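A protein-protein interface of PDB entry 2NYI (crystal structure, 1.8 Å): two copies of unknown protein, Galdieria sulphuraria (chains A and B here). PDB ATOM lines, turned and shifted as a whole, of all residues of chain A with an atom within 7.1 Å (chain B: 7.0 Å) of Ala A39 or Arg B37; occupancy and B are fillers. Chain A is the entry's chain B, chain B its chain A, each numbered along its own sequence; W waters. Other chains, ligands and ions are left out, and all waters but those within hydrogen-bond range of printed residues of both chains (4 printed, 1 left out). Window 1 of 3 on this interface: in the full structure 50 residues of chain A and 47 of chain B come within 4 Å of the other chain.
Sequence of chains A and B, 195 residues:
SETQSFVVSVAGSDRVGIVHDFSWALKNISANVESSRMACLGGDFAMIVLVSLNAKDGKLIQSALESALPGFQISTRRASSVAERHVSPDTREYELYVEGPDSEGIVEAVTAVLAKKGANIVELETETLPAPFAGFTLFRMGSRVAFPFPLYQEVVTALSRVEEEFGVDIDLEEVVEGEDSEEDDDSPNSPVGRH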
ATOM      1  N   VAL A  10     -23.284  -0.784  -6.433  1.00  0.00           N
ATOM      2  CA  VAL A  10     -23.955  -1.104  -7.689  1.00  0.00           C
ATOM      3  C   VAL A  10     -22.901  -1.050  -8.787  1.00  0.00           C
ATOM      4  O   VAL A  10     -22.143  -0.083  -8.866  1.00  0.00           O
ATOM      5  CB  VAL A  10     -25.072  -0.074  -8.007  1.00  0.00           C
ATOM      6  CG1 VAL A  10     -25.809  -0.433  -9.316  1.00  0.00           C
ATOM      7  CG2 VAL A  10     -26.090  -0.005  -6.846  1.00  0.00           C
ATOM      8  N   ASP A  14     -23.064   1.378 -18.116  1.00  0.00           N
ATOM      9  CA  ASP A  14     -23.564   2.737 -18.010  1.00  0.00           C
ATOM     10  C   ASP A  14     -24.696   2.981 -19.010  1.00  0.00           C
ATOM     11  O   ASP A  14     -24.676   2.461 -20.130  1.00  0.00           O
ATOM     12  CB  ASP A  14     -22.447   3.740 -18.258  1.00  0.00           C
ATOM     13  CG  ASP A  14     -22.848   5.133 -17.877  1.00  0.00           C
ATOM     14  OD1 ASP A  14     -23.617   5.280 -16.902  1.00  0.00           O
ATOM     15  OD2 ASP A  14     -22.398   6.081 -18.544  1.00  0.00           O
ATOM     16  N   ARG A  37     -21.214   8.140  -3.896  1.00  0.00           N
ATOM     17  CA  ARG A  37     -20.081   8.450  -4.750  1.00  0.00           C
ATOM     18  C   ARG A  37     -20.211   7.560  -5.973  1.00  0.00           C
ATOM     19  O   ARG A  37     -20.485   6.360  -5.856  1.00  0.00           O
ATOM     20  CB  ARG A  37     -18.753   8.184  -4.022  1.00  0.00           C
ATOM     21  CG  ARG A  37     -18.428   9.275  -2.984  1.00  0.00           C
ATOM     22  CD  ARG A  37     -17.015   9.230  -2.493  1.00  0.00           C
ATOM     23  NE  ARG A  37     -16.690  10.430  -1.722  1.00  0.00           N
ATOM     24  CZ  ARG A  37     -16.183  10.433  -0.490  1.00  0.00           C
ATOM     25  NH1 ARG A  37     -15.912   9.297   0.140  1.00  0.00           N
ATOM     26  NH2 ARG A  37     -15.931  11.587   0.113  1.00  0.00           N
ATOM     27  N   MET A  38     -20.031   8.150  -7.148  1.00  0.00           N
ATOM     28  CA  MET A  38     -20.107   7.392  -8.390  1.00  0.00           C
ATOM     29  C   MET A  38     -18.731   7.313  -9.098  1.00  0.00           C
ATOM     30  O   MET A  38     -17.832   8.137  -8.862  1.00  0.00           O
ATOM     31  CB  MET A  38     -21.136   8.074  -9.286  1.00  0.00           C
ATOM     32  CG  MET A  38     -21.657   7.249 -10.429  1.00  0.00           C
ATOM     33  SD  MET A  38     -22.246   8.495 -11.796  1.00  0.00           S
ATOM     34  CE  MET A  38     -23.983   8.416 -11.476  1.00  0.00           C
ATOM     35  N   ALA A  39     -18.548   6.290  -9.933  1.00  0.00           N
ATOM     36  CA  ALA A  39     -17.453   6.282 -10.908  1.00  0.00           C
ATOM     37  C   ALA A  39     -18.101   5.870 -12.252  1.00  0.00           C
ATOM     38  O   ALA A  39     -18.968   4.996 -12.299  1.00  0.00           O
ATOM     39  CB  ALA A  39     -16.359   5.298 -10.489  1.00  0.00           C
ATOM     40  N   CYS A  40     -17.662   6.512 -13.321  1.00  0.00           N
ATOM     41  CA  CYS A  40     -18.223   6.249 -14.617  1.00  0.00           C
ATOM     42  C   CYS A  40     -17.096   6.397 -15.599  1.00  0.00           C
ATOM     43  O   CYS A  40     -16.407   7.424 -15.590  1.00  0.00           O
ATOM     44  CB  CYS A  40     -19.315   7.268 -14.893  1.00  0.00           C
ATOM     45  SG  CYS A  40     -20.054   7.093 -16.481  1.00  0.00           S
ATOM     46  N   LEU A  41     -16.874   5.362 -16.412  1.00  0.00           N
ATOM     47  CA  LEU A  41     -15.722   5.391 -17.334  1.00  0.00           C
ATOM     48  C   LEU A  41     -15.791   4.253 -18.318  1.00  0.00           C
ATOM     49  O   LEU A  41     -16.144   3.136 -17.948  1.00  0.00           O
ATOM     50  CB  LEU A  41     -14.402   5.312 -16.535  1.00  0.00           C
ATOM     51  CG  LEU A  41     -13.091   5.480 -17.295  1.00  0.00           C
ATOM     52  CD1 LEU A  41     -13.023   6.902 -17.907  1.00  0.00           C
ATOM     53  CD2 LEU A  41     -11.897   5.191 -16.366  1.00  0.00           C
ATOM     54  N   ASP A  44     -18.656   1.700 -18.365  1.00  0.00           N
ATOM     55  CA  ASP A  44     -18.990   1.012 -17.108  1.00  0.00           C
ATOM     56  C   ASP A  44     -19.441   2.047 -16.078  1.00  0.00           C
ATOM     57  O   ASP A  44     -19.045   3.220 -16.148  1.00  0.00           O
ATOM     58  CB  ASP A  44     -17.774   0.261 -16.513  1.00  0.00           C
ATOM     59  CG  ASP A  44     -17.577  -1.144 -17.089  1.00  0.00           C
ATOM     60  OD1 ASP A  44     -18.250  -1.523 -18.082  1.00  0.00           O
ATOM     61  OD2 ASP A  44     -16.712  -1.875 -16.534  1.00  0.00           O
ATOM     62  N   PHE A  45     -20.244   1.588 -15.126  1.00  0.00           N
ATOM     63  CA  PHE A  45     -20.862   2.426 -14.085  1.00  0.00           C
ATOM     64  C   PHE A  45     -20.560   1.752 -12.751  1.00  0.00           C
ATOM     65  O   PHE A  45     -20.648   0.510 -12.632  1.00  0.00           O
ATOM     66  CB  PHE A  45     -22.395   2.470 -14.311  1.00  0.00           C
ATOM     67  CG  PHE A  45     -23.177   3.115 -13.191  1.00  0.00           C
ATOM     68  CD1 PHE A  45     -23.514   4.465 -13.248  1.00  0.00           C
ATOM     69  CD2 PHE A  45     -23.550   2.371 -12.056  1.00  0.00           C
ATOM     70  CE1 PHE A  45     -24.233   5.058 -12.194  1.00  0.00           C
ATOM     71  CE2 PHE A  45     -24.246   2.962 -11.002  1.00  0.00           C
ATOM     72  CZ  PHE A  45     -24.594   4.296 -11.078  1.00  0.00           C
ATOM     73  N   ALA A  46     -20.190   2.554 -11.752  1.00  0.00           N
ATOM     74  CA  ALA A  46     -20.062   2.037 -10.383  1.00  0.00           C
ATOM     75  C   ALA A  46     -20.556   3.117  -9.433  1.00  0.00           C
ATOM     76  O   ALA A  46     -20.326   4.322  -9.660  1.00  0.00           O
ATOM     77  CB  ALA A  46     -18.608   1.674 -10.058  1.00  0.00           C
ATOM     78  N   MET A  47     -21.211   2.698  -8.359  1.00  0.00           N
ATOM     79  CA  MET A  47     -21.699   3.673  -7.386  1.00  0.00           C
ATOM     80  C   MET A  47     -21.752   3.012  -6.021  1.00  0.00           C
ATOM     81  O   MET A  47     -22.084   1.831  -5.914  1.00  0.00           O
ATOM     82  CB  MET A  47     -23.112   4.166  -7.768  1.00  0.00           C
ATOM     83  CG  MET A  47     -23.662   5.132  -6.716  1.00  0.00           C
ATOM     84  SD  MET A  47     -25.228   6.055  -7.403  1.00  0.00           S
ATOM     85  CE  MET A  47     -26.343   4.569  -7.671  1.00  0.00           C
ATOM     86  N   ILE A  48     -21.380   3.764  -4.991  1.00  0.00           N
ATOM     87  CA  ILE A  48     -21.490   3.265  -3.617  1.00  0.00           C
ATOM     88  C   ILE A  48     -22.418   4.257  -2.909  1.00  0.00           C
ATOM     89  O   ILE A  48     -22.292   5.465  -3.089  1.00  0.00           O
ATOM     90  CB  ILE A  48     -20.140   3.234  -2.915  1.00  0.00           C
ATOM     91  CG1 ILE A  48     -19.133   2.376  -3.730  1.00  0.00           C
ATOM     92  CG2 ILE A  48     -20.287   2.708  -1.424  1.00  0.00           C
ATOM     93  CD1 ILE A  48     -17.708   2.454  -3.168  1.00  0.00           C
ATOM     94  N   LEU A 124      -9.604   8.904  -6.018  1.00  0.00           N
ATOM     95  CA  LEU A 124      -8.445   8.780  -6.930  1.00  0.00           C
ATOM     96  C   LEU A 124      -8.932   8.834  -8.346  1.00  0.00           C
ATOM     97  O   LEU A 124      -9.937   8.180  -8.717  1.00  0.00           O
ATOM     98  CB  LEU A 124      -7.683   7.464  -6.681  1.00  0.00           C
ATOM     99  CG  LEU A 124      -6.383   7.246  -7.466  1.00  0.00           C
ATOM    100  CD1 LEU A 124      -5.291   6.658  -6.572  1.00  0.00           C
ATOM    101  CD2 LEU A 124      -6.740   6.337  -8.619  1.00  0.00           C
ATOM    102  N   GLU A 125      -8.247   9.638  -9.144  1.00  0.00           N
ATOM    103  CA  GLU A 125      -8.474   9.557 -10.581  1.00  0.00           C
ATOM    104  C   GLU A 125      -7.179   9.772 -11.339  1.00  0.00           C
ATOM    105  O   GLU A 125      -6.312  10.545 -10.898  1.00  0.00           O
ATOM    106  CB  GLU A 125      -9.626  10.456 -11.032  1.00  0.00           C
ATOM    107  CG  GLU A 125      -9.359  11.911 -11.270  1.00  0.00           C
ATOM    108  CD  GLU A 125     -10.561  12.564 -12.009  1.00  0.00           C
ATOM    109  OE1 GLU A 125     -11.683  12.567 -11.448  1.00  0.00           O
ATOM    110  OE2 GLU A 125     -10.375  13.053 -13.148  1.00  0.00           O
ATOM    111  N   THR A 126      -7.010   9.028 -12.423  1.00  0.00           N
ATOM    112  CA  THR A 126      -5.830   9.220 -13.276  1.00  0.00           C
ATOM    113  C   THR A 126      -6.274   9.403 -14.725  1.00  0.00           C
ATOM    114  O   THR A 126      -7.363   8.963 -15.124  1.00  0.00           O
ATOM    115  CB  THR A 126      -4.819   8.041 -13.190  1.00  0.00           C
ATOM    116  OG1 THR A 126      -5.364   6.905 -13.857  1.00  0.00           O
ATOM    117  CG2 THR A 126      -4.499   7.668 -11.707  1.00  0.00           C
ATOM    118  N   SER B  35      -6.610   5.375 -17.875  1.00  0.00           N
ATOM    119  CA  SER B  35      -7.358   6.285 -16.999  1.00  0.00           C
ATOM    120  C   SER B  35      -8.063   5.466 -15.947  1.00  0.00           C
ATOM    121  O   SER B  35      -8.245   4.267 -16.126  1.00  0.00           O
ATOM    122  CB  SER B  35      -8.366   7.114 -17.800  1.00  0.00           C
ATOM    123  OG  SER B  35      -9.219   6.254 -18.528  1.00  0.00           O
ATOM    124  N   SER B  36      -8.449   6.127 -14.853  1.00  0.00           N
ATOM    125  CA  SER B  36      -9.112   5.438 -13.746  1.00  0.00           C
ATOM    126  C   SER B  36      -9.957   6.399 -12.932  1.00  0.00           C
ATOM    127  O   SER B  36      -9.654   7.606 -12.810  1.00  0.00           O
ATOM    128  CB  SER B  36      -8.096   4.713 -12.858  1.00  0.00           C
ATOM    129  OG  SER B  36      -7.206   5.652 -12.278  1.00  0.00           O
ATOM    130  N   ARG B  37     -11.007   5.856 -12.336  1.00  0.00           N
ATOM    131  CA  ARG B  37     -11.815   6.612 -11.401  1.00  0.00           C
ATOM    132  C   ARG B  37     -12.127   5.672 -10.253  1.00  0.00           C
ATOM    133  O   ARG B  37     -12.610   4.580 -10.478  1.00  0.00           O
ATOM    134  CB  ARG B  37     -13.104   7.059 -12.078  1.00  0.00           C
ATOM    135  CG  ARG B  37     -12.831   8.111 -13.171  1.00  0.00           C
ATOM    136  CD  ARG B  37     -14.064   8.741 -13.734  1.00  0.00           C
ATOM    137  NE  ARG B  37     -13.717   9.923 -14.525  1.00  0.00           N
ATOM    138  CZ  ARG B  37     -14.602  10.703 -15.144  1.00  0.00           C
ATOM    139  NH1 ARG B  37     -15.900  10.428 -15.095  1.00  0.00           N
ATOM    140  NH2 ARG B  37     -14.184  11.759 -15.828  1.00  0.00           N
ATOM    141  N   MET B  38     -11.839   6.104  -9.021  1.00  0.00           N
ATOM    142  CA  MET B  38     -12.028   5.242  -7.856  1.00  0.00           C
ATOM    143  C   MET B  38     -12.807   5.982  -6.787  1.00  0.00           C
ATOM    144  O   MET B  38     -12.511   7.158  -6.483  1.00  0.00           O
ATOM    145  CB  MET B  38     -10.665   4.796  -7.299  1.00  0.00           C
ATOM    146  CG  MET B  38     -10.760   3.951  -6.039  1.00  0.00           C
ATOM    147  SD  MET B  38     -10.112   4.923  -4.446  1.00  0.00           S
ATOM    148  CE  MET B  38     -11.206   5.975  -4.156  1.00  0.00           C
ATOM    149  N   ALA B  39     -13.766   5.269  -6.201  1.00  0.00           N
ATOM    150  CA  ALA B  39     -14.644   5.807  -5.175  1.00  0.00           C
ATOM    151  C   ALA B  39     -14.681   4.847  -4.002  1.00  0.00           C
ATOM    152  O   ALA B  39     -14.699   3.628  -4.171  1.00  0.00           O
ATOM    153  CB  ALA B  39     -16.020   5.996  -5.723  1.00  0.00           C
ATOM    154  N   PHE B  45     -15.360  -0.232  -1.628  1.00  0.00           N
ATOM    155  CA  PHE B  45     -14.409   0.237  -2.629  1.00  0.00           C
ATOM    156  C   PHE B  45     -14.990  -0.064  -4.021  1.00  0.00           C
ATOM    157  O   PHE B  45     -15.493  -1.154  -4.269  1.00  0.00           O
ATOM    158  CB  PHE B  45     -13.039  -0.479  -2.429  1.00  0.00           C
ATOM    159  CG  PHE B  45     -12.063  -0.252  -3.558  1.00  0.00           C
ATOM    160  CD1 PHE B  45     -10.995   0.632  -3.397  1.00  0.00           C
ATOM    161  CD2 PHE B  45     -12.203  -0.926  -4.771  1.00  0.00           C
ATOM    162  CE1 PHE B  45     -10.084   0.850  -4.454  1.00  0.00           C
ATOM    163  CE2 PHE B  45     -11.307  -0.710  -5.836  1.00  0.00           C
ATOM    164  CZ  PHE B  45     -10.248   0.181  -5.665  1.00  0.00           C
ATOM    165  N   ALA B  46     -14.892   0.899  -4.936  1.00  0.00           N
ATOM    166  CA  ALA B  46     -15.245   0.638  -6.345  1.00  0.00           C
ATOM    167  C   ALA B  46     -14.247   1.412  -7.222  1.00  0.00           C
ATOM    168  O   ALA B  46     -13.856   2.561  -6.885  1.00  0.00           O
ATOM    169  CB  ALA B  46     -16.703   1.064  -6.636  1.00  0.00           C
ATOM    170  N   MET B  47     -13.841   0.799  -8.337  1.00  0.00           N
ATOM    171  CA  MET B  47     -12.946   1.472  -9.292  1.00  0.00           C
ATOM    172  C   MET B  47     -13.180   0.966 -10.697  1.00  0.00           C
ATOM    173  O   MET B  47     -13.399  -0.225 -10.907  1.00  0.00           O
ATOM    174  CB  MET B  47     -11.471   1.229  -8.897  1.00  0.00           C
ATOM    175  CG  MET B  47     -10.470   1.909  -9.839  1.00  0.00           C
ATOM    176  SD  MET B  47      -8.681   1.945  -9.050  1.00  0.00           S
ATOM    177  CE  MET B  47      -8.362   0.259  -9.159  1.00  0.00           C
ATOM    178  N   ILE B  48     -13.138   1.884 -11.646  1.00  0.00           N
ATOM    179  CA  ILE B  48     -13.220   1.555 -13.066  1.00  0.00           C
ATOM    180  C   ILE B  48     -11.911   2.053 -13.689  1.00  0.00           C
ATOM    181  O   ILE B  48     -11.442   3.151 -13.379  1.00  0.00           O
ATOM    182  CB  ILE B  48     -14.424   2.204 -13.746  1.00  0.00           C
ATOM    183  CG1 ILE B  48     -15.717   1.811 -13.003  1.00  0.00           C
ATOM    184  CG2 ILE B  48     -14.517   1.722 -15.230  1.00  0.00           C
ATOM    185  CD1 ILE B  48     -16.931   2.637 -13.421  1.00  0.00           C
ATOM    186  N   VAL B  49     -11.311   1.197 -14.513  1.00  0.00           N
ATOM    187  CA  VAL B  49     -10.022   1.498 -15.127  1.00  0.00           C
ATOM    188  C   VAL B  49     -10.062   1.145 -16.621  1.00  0.00           C
ATOM    189  O   VAL B  49     -10.595   0.097 -16.993  1.00  0.00           O
ATOM    190  CB  VAL B  49      -8.902   0.681 -14.447  1.00  0.00           C
ATOM    191  CG1 VAL B  49      -7.523   1.097 -14.968  1.00  0.00           C
ATOM    192  CG2 VAL B  49      -8.957   0.834 -12.896  1.00  0.00           C
ATOM    193  N   LEU B  50      -9.504   2.040 -17.446  1.00  0.00           N
ATOM    194  CA  LEU B  50      -9.204   1.742 -18.856  1.00  0.00           C
ATOM    195  C   LEU B  50      -7.754   1.267 -18.890  1.00  0.00           C
ATOM    196  O   LEU B  50      -6.826   1.975 -18.444  1.00  0.00           O
ATOM    197  CB  LEU B  50      -9.426   2.956 -19.779  1.00  0.00           C
ATOM    198  CG  LEU B  50     -10.905   3.397 -19.902  1.00  0.00           C
ATOM    199  CD1 LEU B  50     -11.056   4.737 -20.602  1.00  0.00           C
ATOM    200  CD2 LEU B  50     -11.686   2.334 -20.661  1.00  0.00           C
ATOM    201  N   GLU B  93     -21.115  19.384 -21.410  1.00  0.00           N
ATOM    202  CA  GLU B  93     -21.106  19.003 -20.012  1.00  0.00           C
ATOM    203  C   GLU B  93     -21.379  20.216 -19.153  1.00  0.00           C
ATOM    204  O   GLU B  93     -21.044  21.362 -19.530  1.00  0.00           O
ATOM    205  CB  GLU B  93     -19.792  18.318 -19.653  1.00  0.00           C
ATOM    206  CG  GLU B  93     -19.615  17.019 -20.420  1.00  0.00           C
ATOM    207  CD  GLU B  93     -18.455  16.176 -19.910  1.00  0.00           C
ATOM    208  OE1 GLU B  93     -17.488  16.742 -19.367  1.00  0.00           O
ATOM    209  OE2 GLU B  93     -18.506  14.940 -20.074  1.00  0.00           O
ATOM    210  N   VAL B 122     -22.144  11.955 -15.420  1.00  0.00           N
ATOM    211  CA  VAL B 122     -20.753  11.559 -15.611  1.00  0.00           C
ATOM    212  C   VAL B 122     -20.041  11.395 -14.261  1.00  0.00           C
ATOM    213  O   VAL B 122     -19.207  10.495 -14.098  1.00  0.00           O
ATOM    214  CB  VAL B 122     -19.996  12.587 -16.496  1.00  0.00           C
ATOM    215  CG1 VAL B 122     -18.580  12.088 -16.789  1.00  0.00           C
ATOM    216  CG2 VAL B 122     -20.759  12.814 -17.801  1.00  0.00           C
ATOM    217  N   GLU B 123     -20.374  12.271 -13.308  1.00  0.00           N
ATOM    218  CA  GLU B 123     -19.775  12.240 -11.956  1.00  0.00           C
ATOM    219  C   GLU B 123     -20.888  12.601 -10.999  1.00  0.00           C
ATOM    220  O   GLU B 123     -21.741  13.409 -11.343  1.00  0.00           O
ATOM    221  CB  GLU B 123     -18.667  13.304 -11.808  1.00  0.00           C
ATOM    222  CG  GLU B 123     -17.639  13.374 -12.945  1.00  0.00           C
ATOM    223  CD  GLU B 123     -16.656  14.551 -12.814  1.00  0.00           C
ATOM    224  OE1 GLU B 123     -16.660  15.245 -11.769  1.00  0.00           O
ATOM    225  OE2 GLU B 123     -15.875  14.775 -13.764  1.00  0.00           O
ATOM    226  N   LEU B 124     -20.880  12.038  -9.781  1.00  0.00           N
ATOM    227  CA  LEU B 124     -21.903  12.392  -8.805  1.00  0.00           C
ATOM    228  C   LEU B 124     -21.373  12.138  -7.414  1.00  0.00           C
ATOM    229  O   LEU B 124     -20.774  11.100  -7.160  1.00  0.00           O
ATOM    230  CB  LEU B 124     -23.189  11.576  -9.028  1.00  0.00           C
ATOM    231  CG  LEU B 124     -24.216  11.673  -7.884  1.00  0.00           C
ATOM    232  CD1 LEU B 124     -24.842  13.031  -7.949  1.00  0.00           C
ATOM    233  CD2 LEU B 124     -25.262  10.595  -7.979  1.00  0.00           C
ATOM    234  N   ARG B 144     -21.466  16.156 -12.423  1.00  0.00           N
ATOM    235  CA  ARG B 144     -21.226  16.554 -13.806  1.00  0.00           C
ATOM    236  C   ARG B 144     -22.184  15.762 -14.682  1.00  0.00           C
ATOM    237  O   ARG B 144     -22.248  14.521 -14.603  1.00  0.00           O
ATOM    238  CB  ARG B 144     -19.780  16.282 -14.196  1.00  0.00           C
ATOM    239  CG  ARG B 144     -19.327  16.932 -15.499  1.00  0.00           C
ATOM    240  CD  ARG B 144     -17.859  16.584 -15.668  1.00  0.00           C
ATOM    241  NE  ARG B 144     -17.206  17.229 -16.799  1.00  0.00           N
ATOM    242  CZ  ARG B 144     -16.308  18.206 -16.694  1.00  0.00           C
ATOM    243  NH1 ARG B 144     -15.964  18.685 -15.503  1.00  0.00           N
ATOM    244  NH2 ARG B 144     -15.758  18.712 -17.791  1.00  0.00           N
HETATM  245  O   HOH W   1     -17.952  10.576  -6.739  1.00  0.00           O
HETATM  246  O   HOH W   2     -17.099   9.399 -12.800  1.00  0.00           O
HETATM  247  O   HOH W   3     -10.375   9.865 -15.297  1.00  0.00           O
HETATM  248  O   HOH W   4     -18.066  11.023  -9.413  1.00  0.00           O
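Hydrophobic or aromatic side chains of chain A that line the printed part of chain B: Met A38, Ala A39, Leu A41, Ala A46, Ile A48 and Leu A124. Along chain B the printed residues that touch a printed residue of chain A span positions 35 to 124. Among the printed residues, 25 pairs touch across the chains. Among the printed residues, no Asp or Glu carboxylate lies within 4 Å of a Lys or Arg side-chain nitrogen of the other chain.
Met A38 touches Leu B124, and with the chains exchanged Leu A124 touches Met B38. Ala A39 touches Ile B48, and with the chains exchanged Ile A48 touches Ala B39. Ala A46 touches its own counterpart, Ala B46. Ala A46 touches Ile B48, and with the chains exchanged Ile A48 touches Ala B46. Positions printed for both chains: 37, 38, 39, 45, 46, 47, 48 and 124. Of the 25 pairs that touch across the chains among the printed residues, 13 have their exchanged pair printed and touching as well.
The backbone carbonyl oxygen of Ser B35 lies within hydrogen-bond range of the backbone NH of Leu B50. The backbone carbonyl oxygen (O) of Val B122 sits at hydrogen-bond distance from the guanidinium group (NH1) of Arg B37 (3.5 Å). The backbone NH (N) of Ala B39 is in hydrogen-bond range of the backbone carbonyl oxygen (O) of Ala B46, at 2.8 Å. The backbone NH (N) of Val B122 sits at hydrogen-bond distance from the backbone carbonyl oxygen (O) of Arg B144, at 2.7 Å. The backbone carbonyl oxygen of Arg A37 is in hydrogen-bond range of the backbone NH of Ile A48, 2.9 Å away. N of Ala A39 is in hydrogen-bond range of O of Ala A46 (2.7 Å).
Among the printed residues, merely in contact across the chains: Arg A37 with Ala B39 (3.9 Å), Arg A37 with Leu B124 (3.6 Å), Ala A39 with Arg B37 (3.8 Å), Ala A39 with Ile B48 (3.3 Å), Cys A40 with Ile B48 (3.9 Å), Cys A40 with Val B122 (3.3 Å), Leu A41 with Ser B35 (3.6 Å), Leu A41 with Ser B36 (3.8 Å), Leu A41 with Ile B48 (3.5 Å), Leu A41 with Leu B50 (3.95 Å), Asp A44 with Ile B48 (3.5 Å), Phe A45 with Ile B48 (3.8 Å), Ala A46 with Ala B46 (3.96 Å), Ala A46 with Ile B48 (3.7 Å), Ile A48 with Ala B39 (3.4 Å), Ile A48 with Phe B45 (3.8 Å), Ile A48 with Ala B46 (3.7 Å), Leu A124 with Ser B36 (3.8 Å), Leu A124 with Arg B37 (3.6 Å), Glu A125 with Ser B36 (3.2 Å) and Thr A126 with Ser B35 (3.3 Å).
Water W2 lies within hydrogen-bond range of the backbone carbonyl oxygen of Val B122, the guanidinium group of Arg B37 and the backbone NH of Cys A40. Water W1 bridges the backbone carbonyl oxygen (O) of Leu B124 (2.9 Å) and the backbone NH (N) of Met A38 (3.2 Å). Water W4 bridges O of Met A38 and N of Leu B124. Water W3 lies within hydrogen-bond range of O of Thr A126 (3.1 Å), NE of Arg B37 (3.4 Å) and O of Ser B36 (3.4 Å).
Of chain B, only Arg B37 and Ile B48 come within 4 Å of Ala A39. Of the printed residues of chain B, Cys A40 touches Arg B37, Ile B48 and Val B122. Of the printed residues of chain B, Asp A44 touches Ile B48. Of the printed residues of chain B, Leu A124 touches Ser B36, Arg B37 and Met B38. Of the printed residues of chain A, Arg B37 touches Ala A39, Cys A40 and Leu A124. Of the printed residues of chain A, Ala B39 touches Arg A37 (3.9 Å) and Ile A48 (3.4 Å). The nearest printed residue of chain A that does not touch Arg B37 is Leu A41 (4.2 Å).
OG1 of Thr A126 lies within hydrogen-bond range of OG of Ser B36, at 2.7 Å. The backbone carbonyl oxygen of Cys A40 is in hydrogen-bond range of the guanidinium group of Arg B37. The backbone carbonyl oxygen (O) of Leu A124 is in hydrogen-bond range of the backbone NH (N) of Met B38. The backbone NH (N) of Met A38 sits at hydrogen-bond distance from the backbone carbonyl oxygen (O) of Leu B124 (3.0 Å).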
